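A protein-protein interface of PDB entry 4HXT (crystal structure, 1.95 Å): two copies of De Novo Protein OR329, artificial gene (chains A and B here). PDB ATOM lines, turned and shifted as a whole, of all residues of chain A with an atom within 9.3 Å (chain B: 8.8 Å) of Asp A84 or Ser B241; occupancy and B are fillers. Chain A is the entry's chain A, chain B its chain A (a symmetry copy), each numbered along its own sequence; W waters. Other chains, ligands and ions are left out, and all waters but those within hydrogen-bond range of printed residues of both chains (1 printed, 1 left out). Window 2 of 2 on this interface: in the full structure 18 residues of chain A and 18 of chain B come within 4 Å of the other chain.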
ATOM      1  N   VAL A  46     -20.194  17.729  -9.129  1.00  0.00           N
ATOM      2  CA  VAL A  46     -20.194  16.563  -8.252  1.00  0.00           C
ATOM      3  C   VAL A  46     -21.486  15.754  -8.381  1.00  0.00           C
ATOM      4  O   VAL A  46     -21.442  14.547  -8.595  1.00  0.00           O
ATOM      5  CB  VAL A  46     -20.001  16.979  -6.774  1.00  0.00           C
ATOM      6  CG1 VAL A  46     -20.170  15.776  -5.853  1.00  0.00           C
ATOM      7  CG2 VAL A  46     -18.632  17.611  -6.588  1.00  0.00           C
ATOM      8  N   GLU A  47     -22.632  16.421  -8.244  1.00  0.00           N
ATOM      9  CA  GLU A  47     -23.927  15.759  -8.351  1.00  0.00           C
ATOM     10  C   GLU A  47     -24.024  15.001  -9.670  1.00  0.00           C
ATOM     11  O   GLU A  47     -24.429  13.842  -9.699  1.00  0.00           O
ATOM     12  CB  GLU A  47     -25.075  16.775  -8.279  1.00  0.00           C
ATOM     13  CG  GLU A  47     -25.452  17.269  -6.884  1.00  0.00           C
ATOM     14  CD  GLU A  47     -24.452  18.255  -6.312  1.00  0.00           C
ATOM     15  OE1 GLU A  47     -23.503  18.637  -7.024  1.00  0.00           O
ATOM     16  OE2 GLU A  47     -24.617  18.657  -5.144  1.00  0.00           O
ATOM     17  N   VAL A  50     -21.648  12.024  -9.811  1.00  0.00           N
ATOM     18  CA  VAL A  50     -22.148  10.951  -8.963  1.00  0.00           C
ATOM     19  C   VAL A  50     -23.224  10.181  -9.715  1.00  0.00           C
ATOM     20  O   VAL A  50     -23.358   8.969  -9.558  1.00  0.00           O
ATOM     21  CB  VAL A  50     -22.725  11.503  -7.638  1.00  0.00           C
ATOM     22  CG1 VAL A  50     -23.528  10.427  -6.919  1.00  0.00           C
ATOM     23  CG2 VAL A  50     -21.581  11.979  -6.748  1.00  0.00           C
ATOM     24  N   ASP A  76     -11.779  20.333   2.065  1.00  0.00           N
ATOM     25  CA  ASP A  76     -12.808  19.583   2.768  1.00  0.00           C
ATOM     26  C   ASP A  76     -14.188  19.904   2.216  1.00  0.00           C
ATOM     27  O   ASP A  76     -15.092  19.079   2.276  1.00  0.00           O
ATOM     28  CB  ASP A  76     -12.765  19.880   4.267  1.00  0.00           C
ATOM     29  CG  ASP A  76     -11.520  19.332   4.934  1.00  0.00           C
ATOM     30  OD1 ASP A  76     -10.939  18.366   4.401  1.00  0.00           O
ATOM     31  OD2 ASP A  76     -11.132  19.853   5.997  1.00  0.00           O
ATOM     32  N   GLU A  77     -14.346  21.106   1.673  1.00  0.00           N
ATOM     33  CA  GLU A  77     -15.623  21.507   1.104  1.00  0.00           C
ATOM     34  C   GLU A  77     -15.929  20.665  -0.131  1.00  0.00           C
ATOM     35  O   GLU A  77     -17.087  20.355  -0.405  1.00  0.00           O
ATOM     36  CB  GLU A  77     -15.617  22.999   0.737  1.00  0.00           C
ATOM     37  CG  GLU A  77     -14.252  23.682   0.805  1.00  0.00           C
ATOM     38  CD  GLU A  77     -13.683  23.731   2.217  1.00  0.00           C
ATOM     39  OE1 GLU A  77     -14.398  24.191   3.133  1.00  0.00           O
ATOM     40  OE2 GLU A  77     -12.521  23.313   2.409  1.00  0.00           O
ATOM     41  N   ALA A  78     -14.886  20.298  -0.874  1.00  0.00           N
ATOM     42  CA  ALA A  78     -15.053  19.473  -2.068  1.00  0.00           C
ATOM     43  C   ALA A  78     -15.512  18.072  -1.642  1.00  0.00           C
ATOM     44  O   ALA A  78     -16.427  17.505  -2.238  1.00  0.00           O
ATOM     45  CB  ALA A  78     -13.739  19.380  -2.832  1.00  0.00           C
ATOM     46  N   ILE A  79     -14.875  17.525  -0.609  1.00  0.00           N
ATOM     47  CA  ILE A  79     -15.217  16.198  -0.095  1.00  0.00           C
ATOM     48  C   ILE A  79     -16.642  16.192   0.448  1.00  0.00           C
ATOM     49  O   ILE A  79     -17.380  15.236   0.259  1.00  0.00           O
ATOM     50  CB  ILE A  79     -14.264  15.758   1.047  1.00  0.00           C
ATOM     51  CG1 ILE A  79     -12.838  15.612   0.510  1.00  0.00           C
ATOM     52  CG2 ILE A  79     -14.753  14.458   1.661  1.00  0.00           C
ATOM     53  CD1 ILE A  79     -11.805  15.288   1.570  1.00  0.00           C
ATOM     54  N   LYS A  80     -17.020  17.269   1.124  1.00  0.00           N
ATOM     55  CA  LYS A  80     -18.345  17.371   1.683  1.00  0.00           C
ATOM     56  C   LYS A  80     -19.399  17.368   0.588  1.00  0.00           C
ATOM     57  O   LYS A  80     -20.484  16.825   0.776  1.00  0.00           O
ATOM     58  CB  LYS A  80     -18.470  18.641   2.506  1.00  0.00           C
ATOM     59  CG  LYS A  80     -19.779  18.735   3.254  1.00  0.00           C
ATOM     60  CD  LYS A  80     -19.804  19.958   4.146  1.00  0.00           C
ATOM     61  CE  LYS A  80     -20.942  19.883   5.116  1.00  0.00           C
ATOM     62  NZ  LYS A  80     -22.217  19.721   4.381  1.00  0.00           N
ATOM     63  N   ALA A  81     -19.078  17.993  -0.544  1.00  0.00           N
ATOM     64  CA  ALA A  81     -19.996  18.056  -1.675  1.00  0.00           C
ATOM     65  C   ALA A  81     -20.263  16.639  -2.175  1.00  0.00           C
ATOM     66  O   ALA A  81     -21.387  16.300  -2.540  1.00  0.00           O
ATOM     67  CB  ALA A  81     -19.403  18.926  -2.798  1.00  0.00           C
ATOM     68  N   ILE A  82     -19.226  15.810  -2.177  1.00  0.00           N
ATOM     69  CA  ILE A  82     -19.367  14.438  -2.634  1.00  0.00           C
ATOM     70  C   ILE A  82     -20.250  13.651  -1.683  1.00  0.00           C
ATOM     71  O   ILE A  82     -21.148  12.937  -2.116  1.00  0.00           O
ATOM     72  CB  ILE A  82     -18.010  13.728  -2.727  1.00  0.00           C
ATOM     73  CG1 ILE A  82     -17.146  14.400  -3.797  1.00  0.00           C
ATOM     74  CG2 ILE A  82     -18.221  12.250  -3.054  1.00  0.00           C
ATOM     75  CD1 ILE A  82     -15.734  13.861  -3.877  1.00  0.00           C
ATOM     76  N   VAL A  83     -19.985  13.783  -0.384  1.00  0.00           N
ATOM     77  CA  VAL A  83     -20.759  13.073   0.626  1.00  0.00           C
ATOM     78  C   VAL A  83     -22.225  13.498   0.625  1.00  0.00           C
ATOM     79  O   VAL A  83     -23.118  12.657   0.665  1.00  0.00           O
ATOM     80  CB  VAL A  83     -20.163  13.293   2.035  1.00  0.00           C
ATOM     81  CG1 VAL A  83     -21.018  12.596   3.080  1.00  0.00           C
ATOM     82  CG2 VAL A  83     -18.728  12.742   2.084  1.00  0.00           C
ATOM     83  N   ASP A  84     -22.473  14.801   0.560  1.00  0.00           N
ATOM     84  CA  ASP A  84     -23.839  15.312   0.561  1.00  0.00           C
ATOM     85  C   ASP A  84     -24.617  14.961  -0.702  1.00  0.00           C
ATOM     86  O   ASP A  84     -25.846  15.060  -0.732  1.00  0.00           O
ATOM     87  CB  ASP A  84     -23.837  16.829   0.770  1.00  0.00           C
ATOM     88  CG  ASP A  84     -23.561  17.220   2.219  1.00  0.00           C
ATOM     89  OD1 ASP A  84     -23.431  16.317   3.078  1.00  0.00           O
ATOM     90  OD2 ASP A  84     -23.481  18.432   2.498  1.00  0.00           O
ATOM     91  N   ALA A  85     -23.903  14.553  -1.744  1.00  0.00           N
ATOM     92  CA  ALA A  85     -24.539  14.173  -3.000  1.00  0.00           C
ATOM     93  C   ALA A  85     -24.753  12.662  -3.015  1.00  0.00           C
ATOM     94  O   ALA A  85     -25.196  12.099  -4.017  1.00  0.00           O
ATOM     95  CB  ALA A  85     -23.671  14.592  -4.180  1.00  0.00           C
ATOM     96  N   GLY A  86     -24.431  12.011  -1.897  1.00  0.00           N
ATOM     97  CA  GLY A  86     -24.602  10.571  -1.796  1.00  0.00           C
ATOM     98  C   GLY A  86     -23.566   9.766  -2.562  1.00  0.00           C
ATOM     99  O   GLY A  86     -23.766   8.584  -2.842  1.00  0.00           O
ATOM    100  N   GLY A  87     -22.448  10.405  -2.892  1.00  0.00           N
ATOM    101  CA  GLY A  87     -21.397   9.738  -3.637  1.00  0.00           C
ATOM    102  C   GLY A  87     -20.703   8.565  -2.967  1.00  0.00           C
ATOM    103  O   GLY A  87     -20.234   7.655  -3.652  1.00  0.00           O
ATOM    104  N   VAL A  88     -20.627   8.574  -1.640  1.00  0.00           N
ATOM    105  CA  VAL A  88     -19.955   7.496  -0.915  1.00  0.00           C
ATOM    106  C   VAL A  88     -20.641   6.136  -1.062  1.00  0.00           C
ATOM    107  O   VAL A  88     -19.993   5.130  -1.349  1.00  0.00           O
ATOM    108  CB  VAL A  88     -19.830   7.845   0.589  1.00  0.00           C
ATOM    109  CG1 VAL A  88     -19.349   6.632   1.372  1.00  0.00           C
ATOM    110  CG2 VAL A  88     -18.851   9.005   0.769  1.00  0.00           C
ATOM    111  N   GLU A  89     -21.955   6.108  -0.868  1.00  0.00           N
ATOM    112  CA  GLU A  89     -22.717   4.866  -0.981  1.00  0.00           C
ATOM    113  C   GLU A  89     -22.532   4.265  -2.378  1.00  0.00           C
ATOM    114  O   GLU A  89     -22.387   3.051  -2.531  1.00  0.00           O
ATOM    115  CB  GLU A  89     -24.198   5.156  -0.702  1.00  0.00           C
ATOM    116  CG  GLU A  89     -25.103   3.941  -0.550  1.00  0.00           C
ATOM    117  CD  GLU A  89     -25.496   3.318  -1.879  1.00  0.00           C
ATOM    118  OE1 GLU A  89     -25.692   4.069  -2.857  1.00  0.00           O
ATOM    119  OE2 GLU A  89     -25.627   2.076  -1.939  1.00  0.00           O
ATOM    120  N   ILE A 113     -11.371  10.563   0.056  1.00  0.00           N
ATOM    121  CA  ILE A 113     -12.458  11.055   0.888  1.00  0.00           C
ATOM    122  C   ILE A 113     -12.073  10.801   2.347  1.00  0.00           C
ATOM    123  O   ILE A 113     -12.254  11.661   3.207  1.00  0.00           O
ATOM    124  CB  ILE A 113     -13.787  10.320   0.561  1.00  0.00           C
ATOM    125  CG1 ILE A 113     -14.315  10.779  -0.802  1.00  0.00           C
ATOM    126  CG2 ILE A 113     -14.816  10.576   1.651  1.00  0.00           C
ATOM    127  CD1 ILE A 113     -15.482   9.955  -1.340  1.00  0.00           C
ATOM    128  N   GLU A 119     -16.219  13.450   9.768  1.00  0.00           N
ATOM    129  CA  GLU A 119     -17.556  13.231   9.226  1.00  0.00           C
ATOM    130  C   GLU A 119     -17.486  12.513   7.883  1.00  0.00           C
ATOM    131  O   GLU A 119     -18.381  11.736   7.544  1.00  0.00           O
ATOM    132  CB  GLU A 119     -18.301  14.559   9.051  1.00  0.00           C
ATOM    133  CG  GLU A 119     -18.694  15.255  10.353  1.00  0.00           C
ATOM    134  CD  GLU A 119     -19.779  14.503  11.119  1.00  0.00           C
ATOM    135  OE1 GLU A 119     -20.536  13.737  10.490  1.00  0.00           O
ATOM    136  OE2 GLU A 119     -19.883  14.690  12.349  1.00  0.00           O
ATOM    137  N   ALA A 120     -16.423  12.760   7.122  1.00  0.00           N
ATOM    138  CA  ALA A 120     -16.268  12.113   5.818  1.00  0.00           C
ATOM    139  C   ALA A 120     -15.973  10.628   6.012  1.00  0.00           C
ATOM    140  O   ALA A 120     -16.492   9.776   5.288  1.00  0.00           O
ATOM    141  CB  ALA A 120     -15.146  12.779   5.023  1.00  0.00           C
ATOM    142  N   ALA A 123     -19.058   8.703   7.019  1.00  0.00           N
ATOM    143  CA  ALA A 123     -19.931   8.418   5.887  1.00  0.00           C
ATOM    144  C   ALA A 123     -19.538   7.081   5.257  1.00  0.00           C
ATOM    145  O   ALA A 123     -20.400   6.263   4.922  1.00  0.00           O
ATOM    146  CB  ALA A 123     -19.837   9.538   4.858  1.00  0.00           C
ATOM    147  N   ALA B 198     -21.196  23.416  14.176  1.00  0.00           N
ATOM    148  CA  ALA B 198     -21.731  23.605  12.833  1.00  0.00           C
ATOM    149  C   ALA B 198     -20.969  22.862  11.728  1.00  0.00           C
ATOM    150  O   ALA B 198     -21.428  22.809  10.585  1.00  0.00           O
ATOM    151  CB  ALA B 198     -21.805  25.104  12.504  1.00  0.00           C
ATOM    152  N   SER B 199     -19.808  22.298  12.047  1.00  0.00           N
ATOM    153  CA  SER B 199     -19.059  21.549  11.042  1.00  0.00           C
ATOM    154  C   SER B 199     -19.407  20.068  11.197  1.00  0.00           C
ATOM    155  O   SER B 199     -18.813  19.202  10.554  1.00  0.00           O
ATOM    156  CB  SER B 199     -17.552  21.745  11.225  1.00  0.00           C
ATOM    157  OG  SER B 199     -17.108  21.170  12.438  1.00  0.00           O
ATOM    158  N   GLY B 200     -20.386  19.791  12.052  1.00  0.00           N
ATOM    159  CA  GLY B 200     -20.793  18.420  12.289  1.00  0.00           C
ATOM    160  C   GLY B 200     -21.943  17.950  11.418  1.00  0.00           C
ATOM    161  O   GLY B 200     -22.105  18.406  10.283  1.00  0.00           O
ATOM    162  N   PRO B 201     -22.778  17.037  11.937  1.00  0.00           N
ATOM    163  CA  PRO B 201     -23.919  16.500  11.195  1.00  0.00           C
ATOM    164  C   PRO B 201     -25.009  17.533  10.970  1.00  0.00           C
ATOM    165  O   PRO B 201     -25.124  18.504  11.714  1.00  0.00           O
ATOM    166  CB  PRO B 201     -24.386  15.353  12.080  1.00  0.00           C
ATOM    167  CG  PRO B 201     -24.153  15.908  13.455  1.00  0.00           C
ATOM    168  CD  PRO B 201     -22.775  16.536  13.326  1.00  0.00           C
ATOM    169  N   THR B 202     -25.811  17.312   9.937  1.00  0.00           N
ATOM    170  CA  THR B 202     -26.903  18.216   9.617  1.00  0.00           C
ATOM    171  C   THR B 202     -27.846  18.365  10.808  1.00  0.00           C
ATOM    172  O   THR B 202     -28.457  19.412  10.992  1.00  0.00           O
ATOM    173  CB  THR B 202     -27.690  17.699   8.398  1.00  0.00           C
ATOM    174  OG1 THR B 202     -26.783  17.502   7.306  1.00  0.00           O
ATOM    175  CG2 THR B 202     -28.768  18.702   7.983  1.00  0.00           C
ATOM    176  N   ILE B 205     -26.856  21.226  12.810  1.00  0.00           N
ATOM    177  CA  ILE B 205     -27.192  22.494  12.163  1.00  0.00           C
ATOM    178  C   ILE B 205     -28.644  22.820  12.491  1.00  0.00           C
ATOM    179  O   ILE B 205     -28.988  23.954  12.821  1.00  0.00           O
ATOM    180  CB  ILE B 205     -27.047  22.409  10.623  1.00  0.00           C
ATOM    181  CG1 ILE B 205     -25.598  22.077  10.253  1.00  0.00           C
ATOM    182  CG2 ILE B 205     -27.475  23.734   9.979  1.00  0.00           C
ATOM    183  CD1 ILE B 205     -24.594  23.101  10.720  1.00  0.00           C
ATOM    184  N   ARG B 234     -17.246  31.824  10.494  1.00  0.00           N
ATOM    185  CA  ARG B 234     -16.993  30.414  10.237  1.00  0.00           C
ATOM    186  C   ARG B 234     -18.264  29.609  10.520  1.00  0.00           C
ATOM    187  O   ARG B 234     -18.636  28.725   9.753  1.00  0.00           O
ATOM    188  CB  ARG B 234     -15.840  29.914  11.114  1.00  0.00           C
ATOM    189  CG  ARG B 234     -15.452  28.455  10.865  1.00  0.00           C
ATOM    190  CD  ARG B 234     -14.053  28.146  11.407  1.00  0.00           C
ATOM    191  NE  ARG B 234     -13.993  28.149  12.866  1.00  0.00           N
ATOM    192  CZ  ARG B 234     -14.306  27.108  13.635  1.00  0.00           C
ATOM    193  NH1 ARG B 234     -14.703  25.969  13.086  1.00  0.00           N
ATOM    194  NH2 ARG B 234     -14.227  27.203  14.954  1.00  0.00           N
ATOM    195  N   ALA B 235     -18.927  29.932  11.623  1.00  0.00           N
ATOM    196  CA  ALA B 235     -20.155  29.241  12.005  1.00  0.00           C
ATOM    197  C   ALA B 235     -21.229  29.434  10.936  1.00  0.00           C
ATOM    198  O   ALA B 235     -21.900  28.480  10.544  1.00  0.00           O
ATOM    199  CB  ALA B 235     -20.645  29.757  13.351  1.00  0.00           C
ATOM    200  N   LEU B 236     -21.377  30.668  10.455  1.00  0.00           N
ATOM    201  CA  LEU B 236     -22.364  30.974   9.425  1.00  0.00           C
ATOM    202  C   LEU B 236     -22.092  30.213   8.131  1.00  0.00           C
ATOM    203  O   LEU B 236     -23.015  29.687   7.504  1.00  0.00           O
ATOM    204  CB  LEU B 236     -22.388  32.481   9.154  1.00  0.00           C
ATOM    205  CG  LEU B 236     -23.028  33.325  10.258  1.00  0.00           C
ATOM    206  CD1 LEU B 236     -22.848  34.806   9.961  1.00  0.00           C
ATOM    207  CD2 LEU B 236     -24.504  32.976  10.362  1.00  0.00           C
ATOM    208  N   GLU B 237     -20.826  30.154   7.725  1.00  0.00           N
ATOM    209  CA  GLU B 237     -20.480  29.426   6.510  1.00  0.00           C
ATOM    210  C   GLU B 237     -20.743  27.929   6.671  1.00  0.00           C
ATOM    211  O   GLU B 237     -21.173  27.260   5.727  1.00  0.00           O
ATOM    212  CB  GLU B 237     -19.015  29.654   6.131  1.00  0.00           C
ATOM    213  CG  GLU B 237     -18.823  30.816   5.177  1.00  0.00           C
ATOM    214  CD  GLU B 237     -17.491  30.764   4.456  1.00  0.00           C
ATOM    215  OE1 GLU B 237     -16.465  31.097   5.081  1.00  0.00           O
ATOM    216  OE2 GLU B 237     -17.472  30.379   3.265  1.00  0.00           O
ATOM    217  N   ASN B 238     -20.485  27.396   7.861  1.00  0.00           N
ATOM    218  CA  ASN B 238     -20.734  25.975   8.087  1.00  0.00           C
ATOM    219  C   ASN B 238     -22.233  25.719   8.014  1.00  0.00           C
ATOM    220  O   ASN B 238     -22.680  24.747   7.413  1.00  0.00           O
ATOM    221  CB  ASN B 238     -20.180  25.528   9.441  1.00  0.00           C
ATOM    222  CG  ASN B 238     -18.669  25.440   9.439  1.00  0.00           C
ATOM    223  OD1 ASN B 238     -18.055  25.376   8.380  1.00  0.00           O
ATOM    224  ND2 ASN B 238     -18.064  25.430  10.620  1.00  0.00           N
ATOM    225  N   ILE B 239     -23.006  26.617   8.609  1.00  0.00           N
ATOM    226  CA  ILE B 239     -24.456  26.488   8.597  1.00  0.00           C
ATOM    227  C   ILE B 239     -24.971  26.502   7.159  1.00  0.00           C
ATOM    228  O   ILE B 239     -25.883  25.752   6.808  1.00  0.00           O
ATOM    229  CB  ILE B 239     -25.106  27.625   9.397  1.00  0.00           C
ATOM    230  CG1 ILE B 239     -24.721  27.487  10.874  1.00  0.00           C
ATOM    231  CG2 ILE B 239     -26.615  27.606   9.205  1.00  0.00           C
ATOM    232  CD1 ILE B 239     -25.123  28.663  11.739  1.00  0.00           C
ATOM    233  N   LYS B 240     -24.371  27.353   6.332  1.00  0.00           N
ATOM    234  CA  LYS B 240     -24.754  27.461   4.930  1.00  0.00           C
ATOM    235  C   LYS B 240     -24.536  26.146   4.184  1.00  0.00           C
ATOM    236  O   LYS B 240     -25.291  25.815   3.274  1.00  0.00           O
ATOM    237  CB  LYS B 240     -23.953  28.577   4.243  1.00  0.00           C
ATOM    238  CG  LYS B 240     -24.236  28.727   2.747  1.00  0.00           C
ATOM    239  CD  LYS B 240     -25.702  29.069   2.488  1.00  0.00           C
ATOM    240  CE  LYS B 240     -25.989  29.262   1.003  1.00  0.00           C
ATOM    241  NZ  LYS B 240     -25.652  28.056   0.201  1.00  0.00           N
ATOM    242  N   SER B 241     -23.501  25.399   4.557  1.00  0.00           N
ATOM    243  CA  SER B 241     -23.231  24.132   3.889  1.00  0.00           C
ATOM    244  C   SER B 241     -24.257  23.082   4.319  1.00  0.00           C
ATOM    245  O   SER B 241     -24.461  22.087   3.628  1.00  0.00           O
ATOM    246  CB  SER B 241     -21.816  23.642   4.206  1.00  0.00           C
ATOM    247  OG  SER B 241     -21.763  23.046   5.482  1.00  0.00           O
ATOM    248  N   GLY B 242     -24.899  23.311   5.461  1.00  0.00           N
ATOM    249  CA  GLY B 242     -25.912  22.386   5.941  1.00  0.00           C
ATOM    250  C   GLY B 242     -25.431  21.203   6.759  1.00  0.00           C
ATOM    251  O   GLY B 242     -26.240  20.369   7.169  1.00  0.00           O
ATOM    252  N   GLY B 243     -24.128  21.124   7.008  1.00  0.00           N
ATOM    253  CA  GLY B 243     -23.601  20.016   7.784  1.00  0.00           C
ATOM    254  C   GLY B 243     -23.506  18.748   6.952  1.00  0.00           C
ATOM    255  O   GLY B 243     -23.826  18.756   5.765  1.00  0.00           O
ATOM    256  N   TRP B 244     -23.071  17.653   7.568  1.00  0.00           N
ATOM    257  CA  TRP B 244     -22.944  16.383   6.858  1.00  0.00           C
ATOM    258  C   TRP B 244     -24.166  15.505   7.106  1.00  0.00           C
ATOM    259  O   TRP B 244     -24.568  15.310   8.253  1.00  0.00           O
ATOM    260  CB  TRP B 244     -21.690  15.636   7.323  1.00  0.00           C
ATOM    261  CG  TRP B 244     -20.433  16.424   7.204  1.00  0.00           C
ATOM    262  CD1 TRP B 244     -20.067  17.504   7.956  1.00  0.00           C
ATOM    263  CD2 TRP B 244     -19.356  16.189   6.289  1.00  0.00           C
ATOM    264  NE1 TRP B 244     -18.827  17.954   7.570  1.00  0.00           N
ATOM    265  CE2 TRP B 244     -18.365  17.160   6.548  1.00  0.00           C
ATOM    266  CE3 TRP B 244     -19.124  15.240   5.279  1.00  0.00           C
ATOM    267  CZ2 TRP B 244     -17.166  17.226   5.827  1.00  0.00           C
ATOM    268  CZ3 TRP B 244     -17.933  15.304   4.562  1.00  0.00           C
ATOM    269  CH2 TRP B 244     -16.967  16.288   4.845  1.00  0.00           C
ATOM    270  N   LEU B 245     -24.760  14.981   6.038  1.00  0.00           N
ATOM    271  CA  LEU B 245     -25.937  14.121   6.175  1.00  0.00           C
ATOM    272  C   LEU B 245     -25.623  12.816   6.919  1.00  0.00           C
ATOM    273  O   LEU B 245     -24.569  12.222   6.724  1.00  0.00           O
ATOM    274  CB  LEU B 245     -26.534  13.826   4.794  1.00  0.00           C
ATOM    275  CG  LEU B 245     -27.141  15.061   4.113  1.00  0.00           C
ATOM    276  CD1 LEU B 245     -27.634  14.716   2.715  1.00  0.00           C
ATOM    277  CD2 LEU B 245     -28.266  15.622   4.976  1.00  0.00           C
ATOM    278  N   GLU B 246     -26.561  12.380   7.757  1.00  0.00           N
ATOM    279  CA  GLU B 246     -26.418  11.176   8.577  1.00  0.00           C
ATOM    280  C   GLU B 246     -26.557   9.817   7.890  1.00  0.00           C
ATOM    281  O   GLU B 246     -26.489   8.795   8.564  1.00  0.00           O
ATOM    282  CB  GLU B 246     -27.413  11.229   9.745  1.00  0.00           C
ATOM    283  CG  GLU B 246     -28.863  11.475   9.339  1.00  0.00           C
ATOM    284  CD  GLU B 246     -29.818  11.424  10.520  1.00  0.00           C
ATOM    285  OE1 GLU B 246     -29.459  11.943  11.599  1.00  0.00           O
ATOM    286  OE2 GLU B 246     -30.930  10.873  10.370  1.00  0.00           O
ATOM    287  N   HIS B 247     -26.756   9.799   6.573  1.00  0.00           N
ATOM    288  CA  HIS B 247     -26.909   8.549   5.817  1.00  0.00           C
ATOM    289  C   HIS B 247     -27.141   7.320   6.701  1.00  0.00           C
ATOM    290  O   HIS B 247     -26.535   6.263   6.423  1.00  0.00           O
ATOM    291  CB  HIS B 247     -25.685   8.311   4.925  1.00  0.00           C
ATOM    292  CG  HIS B 247     -25.408   9.429   3.968  1.00  0.00           C
ATOM    293  ND1 HIS B 247     -26.318   9.840   3.019  1.00  0.00           N
ATOM    294  CD2 HIS B 247     -24.326  10.231   3.830  1.00  0.00           C
ATOM    295  CE1 HIS B 247     -25.807  10.851   2.334  1.00  0.00           C
ATOM    296  NE2 HIS B 247     -24.604  11.106   2.805  1.00  0.00           N
HETATM  297  O   HOH W   1     -22.266  10.074   0.500  1.00  0.00           O
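NZ of Lys A80 is in hydrogen-bond range of O of Ser B241, 3.3 Å away.
NE2 of His B247 sits at hydrogen-bond distance from O of Val A83, 3.0 Å away.
The backbone carbonyl oxygen of Gly B243 sits close to the side-chain amino group of Lys A80 (2.3 Å).
The backbone carbonyl oxygen of Gly B243 lies close to the side-chain carboxylate of Asp A84 (3.3 Å).
The side-chain amino group (NZ) of Lys A80 is in salt-bridge range of the side-chain carboxylate (OD2) of Asp A84, at 2.6 Å.
O of Ser B199 lies within hydrogen-bond range of NE1 of Trp B244 (3.2 Å).
N of Trp B244 sits at hydrogen-bond distance from O of Gly B200 (3.0 Å).
The backbone carbonyl oxygen (O) of Trp B244 sits at hydrogen-bond distance from the backbone NH (N) of Thr B202 (2.9 Å).
OG1 of Thr B202 lies close to N of Leu B245 (3.5 Å).
OG of Ser B241 lies close to N of Gly B243, 3.4 Å away.
Among the printed residues, pairs that only touch across the chains: Glu A119 with Trp B244 (3.4 Å), Asp A84 with Leu B245 (3.5 Å), Glu A119 with Pro B201 (3.6 Å), Lys A80 with Trp B244 (3.6 Å), Val A83 with Trp B244 (3.7 Å), Ala A120 with Trp B244 (3.8 Å), Asp A84 with Trp B244 (3.8 Å), Glu A119 with Gly B200 (3.8 Å), Asp A84 with Ser B241 (3.9 Å) and Glu A119 with Ser B199 (3.95 Å).
Of the printed residues of chain B, Lys A80 touches Ser B241, Gly B243 and Trp B244.
Of chain B, only Ser B241 (3.9 Å), Gly B243 (3.3 Å), Trp B244 (3.8 Å) and Leu B245 (3.5 Å) come within 4 Å of Asp A84.
No residue of chain B comes within 4 Å of Ala A85.
Gly A86 touches none of the printed residues of chain B.
Of the printed residues of chain B, Glu A119 touches Ser B199 (3.95 Å), Gly B200 (3.8 Å), Pro B201 (3.6 Å) and Trp B244 (3.4 Å).
Printed residues of chain A within 4 Å of Ser B199: Glu A119.
Ser B241 touches just these residues of chain A: Lys A80 (3.3 Å) and Asp A84 (3.9 Å).
Gly B243 touches just these residues of chain A: Lys A80 (2.3 Å) and Asp A84 (3.3 Å).
Of the printed residues of chain A, Trp B244 touches Lys A80 (3.6 Å), Val A83 (3.7 Å), Asp A84 (3.8 Å), Glu A119 (3.4 Å) and Ala A120 (3.8 Å).
Glu B246 touches none of the printed residues of chain A.
Of the printed residues of chain A, His B247 touches Val A83 (3.0 Å).
Printed residues of chain A that touch a printed residue of chain B: Lys A80, Val A83, Asp A84, Glu A119 and Ala A120.
Hydrophobic or aromatic side chains of chain A within 4 Å of the printed part of chain B: Val A83 and Ala A120.
Printed residues of chain B that touch a printed residue of chain A: Ser B199, Gly B200, Pro B201, Ser B241, Gly B243, Trp B244, Leu B245 and His B247.
Among the printed residues, 14 pairs touch across the chains.
Among the printed residues, no Asp or Glu carboxylate lies within 4 Å of a Lys or Arg side-chain nitrogen of the other chain.
No position is printed for both chains.
Of the 14 pairs that touch across the chains among the printed residues, none has its exchanged pair printed and touching as well.
Water W1 lies within hydrogen-bond range of O of Val A83 (2.7 Å), N of Val A88 (3.1 Å), N of Gly A87 (3.4 Å) and NE2 of His B247 (3.4 Å).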
